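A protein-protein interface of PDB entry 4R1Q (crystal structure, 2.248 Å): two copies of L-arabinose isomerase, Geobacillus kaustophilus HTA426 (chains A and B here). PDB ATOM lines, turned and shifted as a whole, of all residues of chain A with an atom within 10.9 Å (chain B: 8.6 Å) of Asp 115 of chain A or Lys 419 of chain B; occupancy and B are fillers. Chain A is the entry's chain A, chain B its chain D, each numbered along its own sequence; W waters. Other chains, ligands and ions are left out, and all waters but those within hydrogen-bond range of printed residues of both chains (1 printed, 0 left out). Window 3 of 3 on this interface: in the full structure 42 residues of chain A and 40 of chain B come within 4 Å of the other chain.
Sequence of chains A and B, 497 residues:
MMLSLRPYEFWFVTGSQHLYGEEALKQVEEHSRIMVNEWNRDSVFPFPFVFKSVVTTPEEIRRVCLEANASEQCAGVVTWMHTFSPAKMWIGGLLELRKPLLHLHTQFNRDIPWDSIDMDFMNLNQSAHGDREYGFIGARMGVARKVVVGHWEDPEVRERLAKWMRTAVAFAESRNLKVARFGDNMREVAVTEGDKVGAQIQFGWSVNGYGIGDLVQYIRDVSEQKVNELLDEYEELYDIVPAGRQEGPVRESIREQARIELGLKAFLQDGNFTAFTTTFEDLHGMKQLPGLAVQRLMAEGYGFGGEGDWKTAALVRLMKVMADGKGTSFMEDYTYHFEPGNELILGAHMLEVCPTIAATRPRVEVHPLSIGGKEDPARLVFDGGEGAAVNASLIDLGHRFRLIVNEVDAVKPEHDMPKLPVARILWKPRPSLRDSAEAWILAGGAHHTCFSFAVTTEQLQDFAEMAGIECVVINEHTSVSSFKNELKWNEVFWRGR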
ATOM      1  N   ASP A 111     -19.229  -3.921  17.545  1.00  0.00           N
ATOM      2  CA  ASP A 111     -20.146  -3.377  16.546  1.00  0.00           C
ATOM      3  C   ASP A 111     -19.448  -2.840  15.305  1.00  0.00           C
ATOM      4  O   ASP A 111     -18.313  -2.380  15.372  1.00  0.00           O
ATOM      5  CB  ASP A 111     -20.973  -2.232  17.156  1.00  0.00           C
ATOM      6  CG  ASP A 111     -21.964  -2.711  18.211  1.00  0.00           C
ATOM      7  OD1 ASP A 111     -22.189  -3.937  18.339  1.00  0.00           O
ATOM      8  OD2 ASP A 111     -22.525  -1.855  18.916  1.00  0.00           O
ATOM      9  N   ILE A 112     -20.148  -2.875  14.177  1.00  0.00           N
ATOM     10  CA  ILE A 112     -19.654  -2.253  12.961  1.00  0.00           C
ATOM     11  C   ILE A 112     -19.736  -0.739  13.126  1.00  0.00           C
ATOM     12  O   ILE A 112     -20.804  -0.219  13.436  1.00  0.00           O
ATOM     13  CB  ILE A 112     -20.486  -2.673  11.733  1.00  0.00           C
ATOM     14  CG1 ILE A 112     -20.208  -4.138  11.374  1.00  0.00           C
ATOM     15  CG2 ILE A 112     -20.216  -1.738  10.542  1.00  0.00           C
ATOM     16  CD1 ILE A 112     -21.147  -4.714  10.314  1.00  0.00           C
ATOM     17  N   PRO A 113     -18.598  -0.033  12.947  1.00  0.00           N
ATOM     18  CA  PRO A 113     -18.569   1.438  12.985  1.00  0.00           C
ATOM     19  C   PRO A 113     -19.037   1.994  11.639  1.00  0.00           C
ATOM     20  O   PRO A 113     -18.219   2.320  10.777  1.00  0.00           O
ATOM     21  CB  PRO A 113     -17.087   1.760  13.238  1.00  0.00           C
ATOM     22  CG  PRO A 113     -16.347   0.597  12.628  1.00  0.00           C
ATOM     23  CD  PRO A 113     -17.253  -0.616  12.776  1.00  0.00           C
ATOM     24  N   TRP A 114     -20.354   2.083  11.473  1.00  0.00           N
ATOM     25  CA  TRP A 114     -20.961   2.370  10.177  1.00  0.00           C
ATOM     26  C   TRP A 114     -20.376   3.596   9.470  1.00  0.00           C
ATOM     27  O   TRP A 114     -20.052   3.541   8.281  1.00  0.00           O
ATOM     28  CB  TRP A 114     -22.470   2.547  10.330  1.00  0.00           C
ATOM     29  CG  TRP A 114     -23.151   1.445  11.114  1.00  0.00           C
ATOM     30  CD1 TRP A 114     -23.591   1.508  12.405  1.00  0.00           C
ATOM     31  CD2 TRP A 114     -23.466   0.127  10.646  1.00  0.00           C
ATOM     32  NE1 TRP A 114     -24.164   0.311  12.772  1.00  0.00           N
ATOM     33  CE2 TRP A 114     -24.098  -0.554  11.710  1.00  0.00           C
ATOM     34  CE3 TRP A 114     -23.278  -0.542   9.431  1.00  0.00           C
ATOM     35  CZ2 TRP A 114     -24.544  -1.871  11.594  1.00  0.00           C
ATOM     36  CZ3 TRP A 114     -23.722  -1.848   9.316  1.00  0.00           C
ATOM     37  CH2 TRP A 114     -24.351  -2.496  10.393  1.00  0.00           C
ATOM     38  N   ASP A 115     -20.229   4.695  10.199  1.00  0.00           N
ATOM     39  CA  ASP A 115     -19.864   5.961   9.565  1.00  0.00           C
ATOM     40  C   ASP A 115     -18.392   6.041   9.135  1.00  0.00           C
ATOM     41  O   ASP A 115     -18.041   6.882   8.312  1.00  0.00           O
ATOM     42  CB  ASP A 115     -20.240   7.145  10.465  1.00  0.00           C
ATOM     43  CG  ASP A 115     -19.434   7.180  11.751  1.00  0.00           C
ATOM     44  OD1 ASP A 115     -18.790   6.154  12.078  1.00  0.00           O
ATOM     45  OD2 ASP A 115     -19.453   8.227  12.442  1.00  0.00           O
ATOM     46  N   SER A 116     -17.546   5.157   9.670  1.00  0.00           N
ATOM     47  CA  SER A 116     -16.113   5.178   9.355  1.00  0.00           C
ATOM     48  C   SER A 116     -15.542   3.890   8.737  1.00  0.00           C
ATOM     49  O   SER A 116     -14.388   3.872   8.305  1.00  0.00           O
ATOM     50  CB  SER A 116     -15.310   5.508  10.605  1.00  0.00           C
ATOM     51  OG  SER A 116     -15.475   4.490  11.559  1.00  0.00           O
ATOM     52  N   ILE A 117     -16.323   2.812   8.698  1.00  0.00           N
ATOM     53  CA  ILE A 117     -15.789   1.551   8.190  1.00  0.00           C
ATOM     54  C   ILE A 117     -15.318   1.667   6.737  1.00  0.00           C
ATOM     55  O   ILE A 117     -16.020   2.196   5.880  1.00  0.00           O
ATOM     56  CB  ILE A 117     -16.775   0.368   8.347  1.00  0.00           C
ATOM     57  CG1 ILE A 117     -16.122  -0.922   7.840  1.00  0.00           C
ATOM     58  CG2 ILE A 117     -18.104   0.661   7.629  1.00  0.00           C
ATOM     59  CD1 ILE A 117     -16.951  -2.184   8.038  1.00  0.00           C
ATOM     60  N   ASP A 118     -14.107   1.177   6.488  1.00  0.00           N
ATOM     61  CA  ASP A 118     -13.460   1.297   5.199  1.00  0.00           C
ATOM     62  C   ASP A 118     -12.661   0.029   4.886  1.00  0.00           C
ATOM     63  O   ASP A 118     -12.745  -0.968   5.616  1.00  0.00           O
ATOM     64  CB  ASP A 118     -12.556   2.545   5.162  1.00  0.00           C
ATOM     65  CG  ASP A 118     -11.430   2.521   6.226  1.00  0.00           C
ATOM     66  OD1 ASP A 118     -11.089   1.441   6.775  1.00  0.00           O
ATOM     67  OD2 ASP A 118     -10.862   3.607   6.497  1.00  0.00           O
ATOM     68  N   MET A 119     -11.873   0.071   3.818  1.00  0.00           N
ATOM     69  CA  MET A 119     -11.106  -1.103   3.425  1.00  0.00           C
ATOM     70  C   MET A 119     -10.056  -1.558   4.459  1.00  0.00           C
ATOM     71  O   MET A 119      -9.874  -2.754   4.664  1.00  0.00           O
ATOM     72  CB  MET A 119     -10.493  -0.931   2.040  1.00  0.00           C
ATOM     73  CG  MET A 119     -10.279  -2.270   1.340  1.00  0.00           C
ATOM     74  SD  MET A 119     -11.842  -3.187   1.174  1.00  0.00           S
ATOM     75  CE  MET A 119     -11.203  -4.822   0.789  1.00  0.00           C
ATOM     76  N   ASP A 120      -9.377  -0.619   5.114  1.00  0.00           N
ATOM     77  CA  ASP A 120      -8.432  -0.989   6.174  1.00  0.00           C
ATOM     78  C   ASP A 120      -9.120  -1.705   7.339  1.00  0.00           C
ATOM     79  O   ASP A 120      -8.561  -2.653   7.898  1.00  0.00           O
ATOM     80  CB  ASP A 120      -7.676   0.227   6.708  1.00  0.00           C
ATOM     81  CG  ASP A 120      -6.568   0.684   5.769  1.00  0.00           C
ATOM     82  OD1 ASP A 120      -6.006  -0.164   5.035  1.00  0.00           O
ATOM     83  OD2 ASP A 120      -6.254   1.893   5.773  1.00  0.00           O
ATOM     84  N   PHE A 121     -10.319  -1.243   7.706  1.00  0.00           N
ATOM     85  CA  PHE A 121     -11.111  -1.917   8.733  1.00  0.00           C
ATOM     86  C   PHE A 121     -11.446  -3.336   8.283  1.00  0.00           C
ATOM     87  O   PHE A 121     -11.311  -4.285   9.056  1.00  0.00           O
ATOM     88  CB  PHE A 121     -12.396  -1.146   9.050  1.00  0.00           C
ATOM     89  CG  PHE A 121     -13.117  -1.648  10.282  1.00  0.00           C
ATOM     90  CD1 PHE A 121     -14.048  -2.680  10.197  1.00  0.00           C
ATOM     91  CD2 PHE A 121     -12.855  -1.095  11.529  1.00  0.00           C
ATOM     92  CE1 PHE A 121     -14.705  -3.147  11.333  1.00  0.00           C
ATOM     93  CE2 PHE A 121     -13.510  -1.558  12.665  1.00  0.00           C
ATOM     94  CZ  PHE A 121     -14.433  -2.576  12.569  1.00  0.00           C
ATOM     95  N   MET A 122     -11.869  -3.467   7.026  1.00  0.00           N
ATOM     96  CA  MET A 122     -12.240  -4.763   6.458  1.00  0.00           C
ATOM     97  C   MET A 122     -11.060  -5.727   6.406  1.00  0.00           C
ATOM     98  O   MET A 122     -11.237  -6.929   6.627  1.00  0.00           O
ATOM     99  CB  MET A 122     -12.854  -4.610   5.060  1.00  0.00           C
ATOM    100  CG  MET A 122     -14.098  -3.734   5.027  1.00  0.00           C
ATOM    101  SD  MET A 122     -15.643  -4.587   5.392  1.00  0.00           S
ATOM    102  CE  MET A 122     -15.933  -5.369   3.798  1.00  0.00           C
ATOM    103  N   ASN A 123      -9.865  -5.216   6.109  1.00  0.00           N
ATOM    104  CA  ASN A 123      -8.680  -6.072   6.064  1.00  0.00           C
ATOM    105  C   ASN A 123      -8.300  -6.559   7.451  1.00  0.00           C
ATOM    106  O   ASN A 123      -7.802  -7.670   7.627  1.00  0.00           O
ATOM    107  CB  ASN A 123      -7.491  -5.336   5.465  1.00  0.00           C
ATOM    108  CG  ASN A 123      -7.656  -5.070   4.002  1.00  0.00           C
ATOM    109  OD1 ASN A 123      -8.532  -5.647   3.343  1.00  0.00           O
ATOM    110  ND2 ASN A 123      -6.806  -4.197   3.466  1.00  0.00           N
ATOM    111  N   ARG B 363     -23.599   2.298  -8.292  1.00  0.00           N
ATOM    112  CA  ARG B 363     -22.756   3.409  -8.712  1.00  0.00           C
ATOM    113  C   ARG B 363     -21.391   2.896  -9.172  1.00  0.00           C
ATOM    114  O   ARG B 363     -20.808   2.015  -8.539  1.00  0.00           O
ATOM    115  CB  ARG B 363     -22.608   4.482  -7.618  1.00  0.00           C
ATOM    116  CG  ARG B 363     -21.704   5.665  -8.073  1.00  0.00           C
ATOM    117  CD  ARG B 363     -21.900   6.983  -7.288  1.00  0.00           C
ATOM    118  NE  ARG B 363     -21.541   6.864  -5.872  1.00  0.00           N
ATOM    119  CZ  ARG B 363     -20.857   7.777  -5.179  1.00  0.00           C
ATOM    120  NH1 ARG B 363     -20.435   8.892  -5.764  1.00  0.00           N
ATOM    121  NH2 ARG B 363     -20.586   7.572  -3.896  1.00  0.00           N
ATOM    122  N   GLU B 365     -17.642   3.403  -9.304  1.00  0.00           N
ATOM    123  CA  GLU B 365     -16.646   4.133  -8.544  1.00  0.00           C
ATOM    124  C   GLU B 365     -15.252   3.565  -8.772  1.00  0.00           C
ATOM    125  O   GLU B 365     -15.083   2.404  -9.146  1.00  0.00           O
ATOM    126  CB  GLU B 365     -16.996   4.101  -7.062  1.00  0.00           C
ATOM    127  CG  GLU B 365     -18.423   4.512  -6.791  1.00  0.00           C
ATOM    128  CD  GLU B 365     -18.745   4.586  -5.314  1.00  0.00           C
ATOM    129  OE1 GLU B 365     -17.825   4.405  -4.490  1.00  0.00           O
ATOM    130  OE2 GLU B 365     -19.925   4.824  -4.980  1.00  0.00           O
ATOM    131  N   HIS B 367     -11.504   3.396  -6.809  1.00  0.00           N
ATOM    132  CA  HIS B 367     -10.837   3.544  -5.520  1.00  0.00           C
ATOM    133  C   HIS B 367      -9.525   2.783  -5.560  1.00  0.00           C
ATOM    134  O   HIS B 367      -9.399   1.814  -6.297  1.00  0.00           O
ATOM    135  CB  HIS B 367     -11.693   2.953  -4.395  1.00  0.00           C
ATOM    136  CG  HIS B 367     -12.965   3.697  -4.138  1.00  0.00           C
ATOM    137  ND1 HIS B 367     -12.994   4.939  -3.543  1.00  0.00           N
ATOM    138  CD2 HIS B 367     -14.254   3.367  -4.388  1.00  0.00           C
ATOM    139  CE1 HIS B 367     -14.248   5.345  -3.442  1.00  0.00           C
ATOM    140  NE2 HIS B 367     -15.031   4.411  -3.950  1.00  0.00           N
ATOM    141  N   VAL B 381     -20.751  -0.276  -6.816  1.00  0.00           N
ATOM    142  CA  VAL B 381     -20.990  -0.110  -5.387  1.00  0.00           C
ATOM    143  C   VAL B 381     -22.486   0.049  -5.120  1.00  0.00           C
ATOM    144  O   VAL B 381     -23.173   0.800  -5.818  1.00  0.00           O
ATOM    145  CB  VAL B 381     -20.281   1.135  -4.839  1.00  0.00           C
ATOM    146  CG1 VAL B 381     -20.506   1.246  -3.326  1.00  0.00           C
ATOM    147  CG2 VAL B 381     -18.793   1.075  -5.158  1.00  0.00           C
ATOM    148  N   HIS B 415     -27.983   2.151   8.637  1.00  0.00           N
ATOM    149  CA  HIS B 415     -27.012   3.243   8.536  1.00  0.00           C
ATOM    150  C   HIS B 415     -26.239   3.269   7.227  1.00  0.00           C
ATOM    151  O   HIS B 415     -25.952   2.224   6.626  1.00  0.00           O
ATOM    152  CB  HIS B 415     -26.002   3.191   9.683  1.00  0.00           C
ATOM    153  CG  HIS B 415     -26.626   3.239  11.040  1.00  0.00           C
ATOM    154  ND1 HIS B 415     -26.854   2.108  11.795  1.00  0.00           N
ATOM    155  CD2 HIS B 415     -27.071   4.284  11.779  1.00  0.00           C
ATOM    156  CE1 HIS B 415     -27.406   2.453  12.944  1.00  0.00           C
ATOM    157  NE2 HIS B 415     -27.546   3.768  12.960  1.00  0.00           N
ATOM    158  N   ASP B 416     -25.886   4.476   6.799  1.00  0.00           N
ATOM    159  CA  ASP B 416     -25.014   4.637   5.652  1.00  0.00           C
ATOM    160  C   ASP B 416     -23.595   4.176   5.977  1.00  0.00           C
ATOM    161  O   ASP B 416     -23.158   4.228   7.122  1.00  0.00           O
ATOM    162  CB  ASP B 416     -25.004   6.097   5.188  1.00  0.00           C
ATOM    163  CG  ASP B 416     -26.290   6.488   4.476  1.00  0.00           C
ATOM    164  OD1 ASP B 416     -26.935   5.597   3.883  1.00  0.00           O
ATOM    165  OD2 ASP B 416     -26.658   7.680   4.506  1.00  0.00           O
ATOM    166  N   MET B 417     -22.889   3.727   4.951  1.00  0.00           N
ATOM    167  CA  MET B 417     -21.484   3.353   5.074  1.00  0.00           C
ATOM    168  C   MET B 417     -20.671   4.126   4.041  1.00  0.00           C
ATOM    169  O   MET B 417     -20.250   3.566   3.029  1.00  0.00           O
ATOM    170  CB  MET B 417     -21.321   1.847   4.893  1.00  0.00           C
ATOM    171  CG  MET B 417     -21.694   1.060   6.142  1.00  0.00           C
ATOM    172  SD  MET B 417     -21.842  -0.729   5.901  1.00  0.00           S
ATOM    173  CE  MET B 417     -23.449  -0.849   5.135  1.00  0.00           C
ATOM    174  N   PRO B 418     -20.459   5.429   4.298  1.00  0.00           N
ATOM    175  CA  PRO B 418     -19.901   6.382   3.330  1.00  0.00           C
ATOM    176  C   PRO B 418     -18.443   6.101   2.995  1.00  0.00           C
ATOM    177  O   PRO B 418     -17.982   6.472   1.918  1.00  0.00           O
ATOM    178  CB  PRO B 418     -20.010   7.736   4.052  1.00  0.00           C
ATOM    179  CG  PRO B 418     -20.814   7.493   5.274  1.00  0.00           C
ATOM    180  CD  PRO B 418     -20.675   6.048   5.611  1.00  0.00           C
ATOM    181  N   LYS B 419     -17.724   5.447   3.898  1.00  0.00           N
ATOM    182  CA  LYS B 419     -16.298   5.238   3.685  1.00  0.00           C
ATOM    183  C   LYS B 419     -15.980   3.857   3.107  1.00  0.00           C
ATOM    184  O   LYS B 419     -14.821   3.517   2.908  1.00  0.00           O
ATOM    185  CB  LYS B 419     -15.532   5.485   4.990  1.00  0.00           C
ATOM    186  CG  LYS B 419     -15.820   6.841   5.602  1.00  0.00           C
ATOM    187  CD  LYS B 419     -15.121   7.960   4.843  1.00  0.00           C
ATOM    188  CE  LYS B 419     -13.631   8.001   5.222  1.00  0.00           C
ATOM    189  NZ  LYS B 419     -12.818   8.935   4.377  1.00  0.00           N
ATOM    190  N   LEU B 420     -17.017   3.069   2.836  1.00  0.00           N
ATOM    191  CA  LEU B 420     -16.834   1.698   2.368  1.00  0.00           C
ATOM    192  C   LEU B 420     -16.883   1.655   0.851  1.00  0.00           C
ATOM    193  O   LEU B 420     -17.922   1.957   0.263  1.00  0.00           O
ATOM    194  CB  LEU B 420     -17.924   0.796   2.942  1.00  0.00           C
ATOM    195  CG  LEU B 420     -17.739  -0.700   2.697  1.00  0.00           C
ATOM    196  CD1 LEU B 420     -16.510  -1.214   3.434  1.00  0.00           C
ATOM    197  CD2 LEU B 420     -18.987  -1.480   3.111  1.00  0.00           C
ATOM    198  N   PRO B 421     -15.760   1.281   0.211  1.00  0.00           N
ATOM    199  CA  PRO B 421     -15.601   1.370  -1.251  1.00  0.00           C
ATOM    200  C   PRO B 421     -16.098   0.154  -2.044  1.00  0.00           C
ATOM    201  O   PRO B 421     -15.889   0.106  -3.246  1.00  0.00           O
ATOM    202  CB  PRO B 421     -14.085   1.488  -1.412  1.00  0.00           C
ATOM    203  CG  PRO B 421     -13.558   0.657  -0.297  1.00  0.00           C
ATOM    204  CD  PRO B 421     -14.491   0.906   0.868  1.00  0.00           C
ATOM    205  N   VAL B 422     -16.733  -0.811  -1.391  1.00  0.00           N
ATOM    206  CA  VAL B 422     -17.233  -1.990  -2.086  1.00  0.00           C
ATOM    207  C   VAL B 422     -18.718  -2.178  -1.826  1.00  0.00           C
ATOM    208  O   VAL B 422     -19.235  -1.718  -0.809  1.00  0.00           O
ATOM    209  CB  VAL B 422     -16.488  -3.271  -1.641  1.00  0.00           C
ATOM    210  CG1 VAL B 422     -15.027  -3.190  -2.044  1.00  0.00           C
ATOM    211  CG2 VAL B 422     -16.629  -3.485  -0.114  1.00  0.00           C
ATOM    212  N   ARG B 424     -21.883  -4.336  -0.684  1.00  0.00           N
ATOM    213  CA  ARG B 424     -21.988  -5.202   0.484  1.00  0.00           C
ATOM    214  C   ARG B 424     -23.439  -5.558   0.757  1.00  0.00           C
ATOM    215  O   ARG B 424     -24.350  -4.885   0.274  1.00  0.00           O
ATOM    216  CB  ARG B 424     -21.364  -4.530   1.718  1.00  0.00           C
ATOM    217  CG  ARG B 424     -22.242  -3.518   2.455  1.00  0.00           C
ATOM    218  CD  ARG B 424     -22.752  -2.379   1.566  1.00  0.00           C
ATOM    219  NE  ARG B 424     -21.671  -1.600   0.975  1.00  0.00           N
ATOM    220  CZ  ARG B 424     -21.664  -0.266   0.876  1.00  0.00           C
ATOM    221  NH1 ARG B 424     -20.629   0.347   0.318  1.00  0.00           N
ATOM    222  NH2 ARG B 424     -22.680   0.464   1.339  1.00  0.00           N
HETATM  223  O   HOH W   1     -18.235   3.754   5.985  1.00  0.00           O
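Water W1 lies within hydrogen-bond range of the backbone carbonyl oxygen of Ile 117 of chain A (2.7 Å), the backbone NH of Lys 419 of chain B (2.7 Å), the backbone carbonyl oxygen of Trp 114 of chain A (2.9 Å) and the backbone NH of Leu 420 of chain B (3.4 Å).
Trp 114 of chain A touches Met 417 of chain B (O to CA, 3.5 Å).
Trp 114 of chain A touches Pro 418 of chain B (O to CD, 3.7 Å).
Asp 115 of chain A touches Pro 418 of chain B.
O of Asp 115 of chain A touches CG of Lys 419 of chain B, at 3.5 Å.
Lys 419 of chain B touches Ser 116 of chain A (CB to O, 3.9 Å).
Ile 117 of chain A touches Met 417 of chain B.
CB of Asp 118 of chain A touches O of Lys 419 of chain B, 3.3 Å away.
Leu 420 of chain B touches Met 122 of chain A.
O of Trp 114 of chain A sits close to O of Asp 416 of chain B.
The backbone carbonyl oxygen of Ile 117 of chain A sits at hydrogen-bond distance from the backbone NH of Leu 420 of chain B (3.3 Å).
The indole nitrogen (NE1) of Trp 114 of chain A sits close to a ring nitrogen (ND1) of His 415 of chain B (3.4 Å).
The backbone carbonyl oxygen of Ile 117 of chain A lies close to the backbone carbonyl oxygen of Lys 419 of chain B (3.5 Å).
Printed residues of chain B within 4 Å of Trp 114 of chain A: His 415, Asp 416, Met 417 and Pro 418.
Asp 115 of chain A touches just these residues of chain B: Pro 418 (3.9 Å) and Lys 419 (3.5 Å).
Of chain B, only Lys 419 (3.9 Å) comes within 4 Å of Ser 116 of chain A.
Printed residues of chain B within 4 Å of Ile 117 of chain A: Met 417 (3.9 Å), Lys 419 (3.2 Å) and Leu 420 (3.3 Å).
Met 119 of chain A touches none of the printed residues of chain B.
Of the printed residues of chain B, Met 122 of chain A touches Leu 420 (3.8 Å).
Val 381 of chain B touches none of the printed residues of chain A.
Printed residues of chain A within 4 Å of Asp 416 of chain B: Trp 114.
Printed residues of chain A within 4 Å of Met 417 of chain B: Trp 114 (3.5 Å) and Ile 117 (3.9 Å).
Pro 418 of chain B touches two residues of chain A.
Lys 419 of chain B touches just these residues of chain A: Asp 115 (3.5 Å), Ser 116 (3.9 Å), Ile 117 (3.2 Å) and Asp 118 (3.3 Å).
Of chain A, only Ile 117 and Met 122 come within 4 Å of Leu 420 of chain B.
The nearest residue of chain B that does not touch Asp 115 of chain A is Asp 416 of chain B (4.3 Å).
The nearest residue of chain A that does not touch Lys 419 of chain B is Met 119 of chain A (4.6 Å).
No position is printed for both chains.
Of the 13 printed residues of chain B, 6 touch a printed residue of chain A.
Hydrophobic or aromatic side chains of chain B that line the printed part of chain A: His 415, Met 417, Pro 418 and Leu 420.
Of the 13 printed residues of chain A, 6 touch a printed residue of chain B.
The backbone NH of Phe 121 of chain A lies within hydrogen-bond range of the side-chain carboxylate of Asp 118 of chain A, 2.9 Å away.
The side-chain carboxylate of Asp 118 of chain A is in hydrogen-bond range of the backbone NH of Asp 120 of chain A.
The guanidinium group of Arg 424 of chain B lies within hydrogen-bond range of the backbone carbonyl oxygen of Leu 420 of chain B (3.2 Å).
NE1 of Trp 114 of chain A lies close to O of Ile 112 of chain A.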
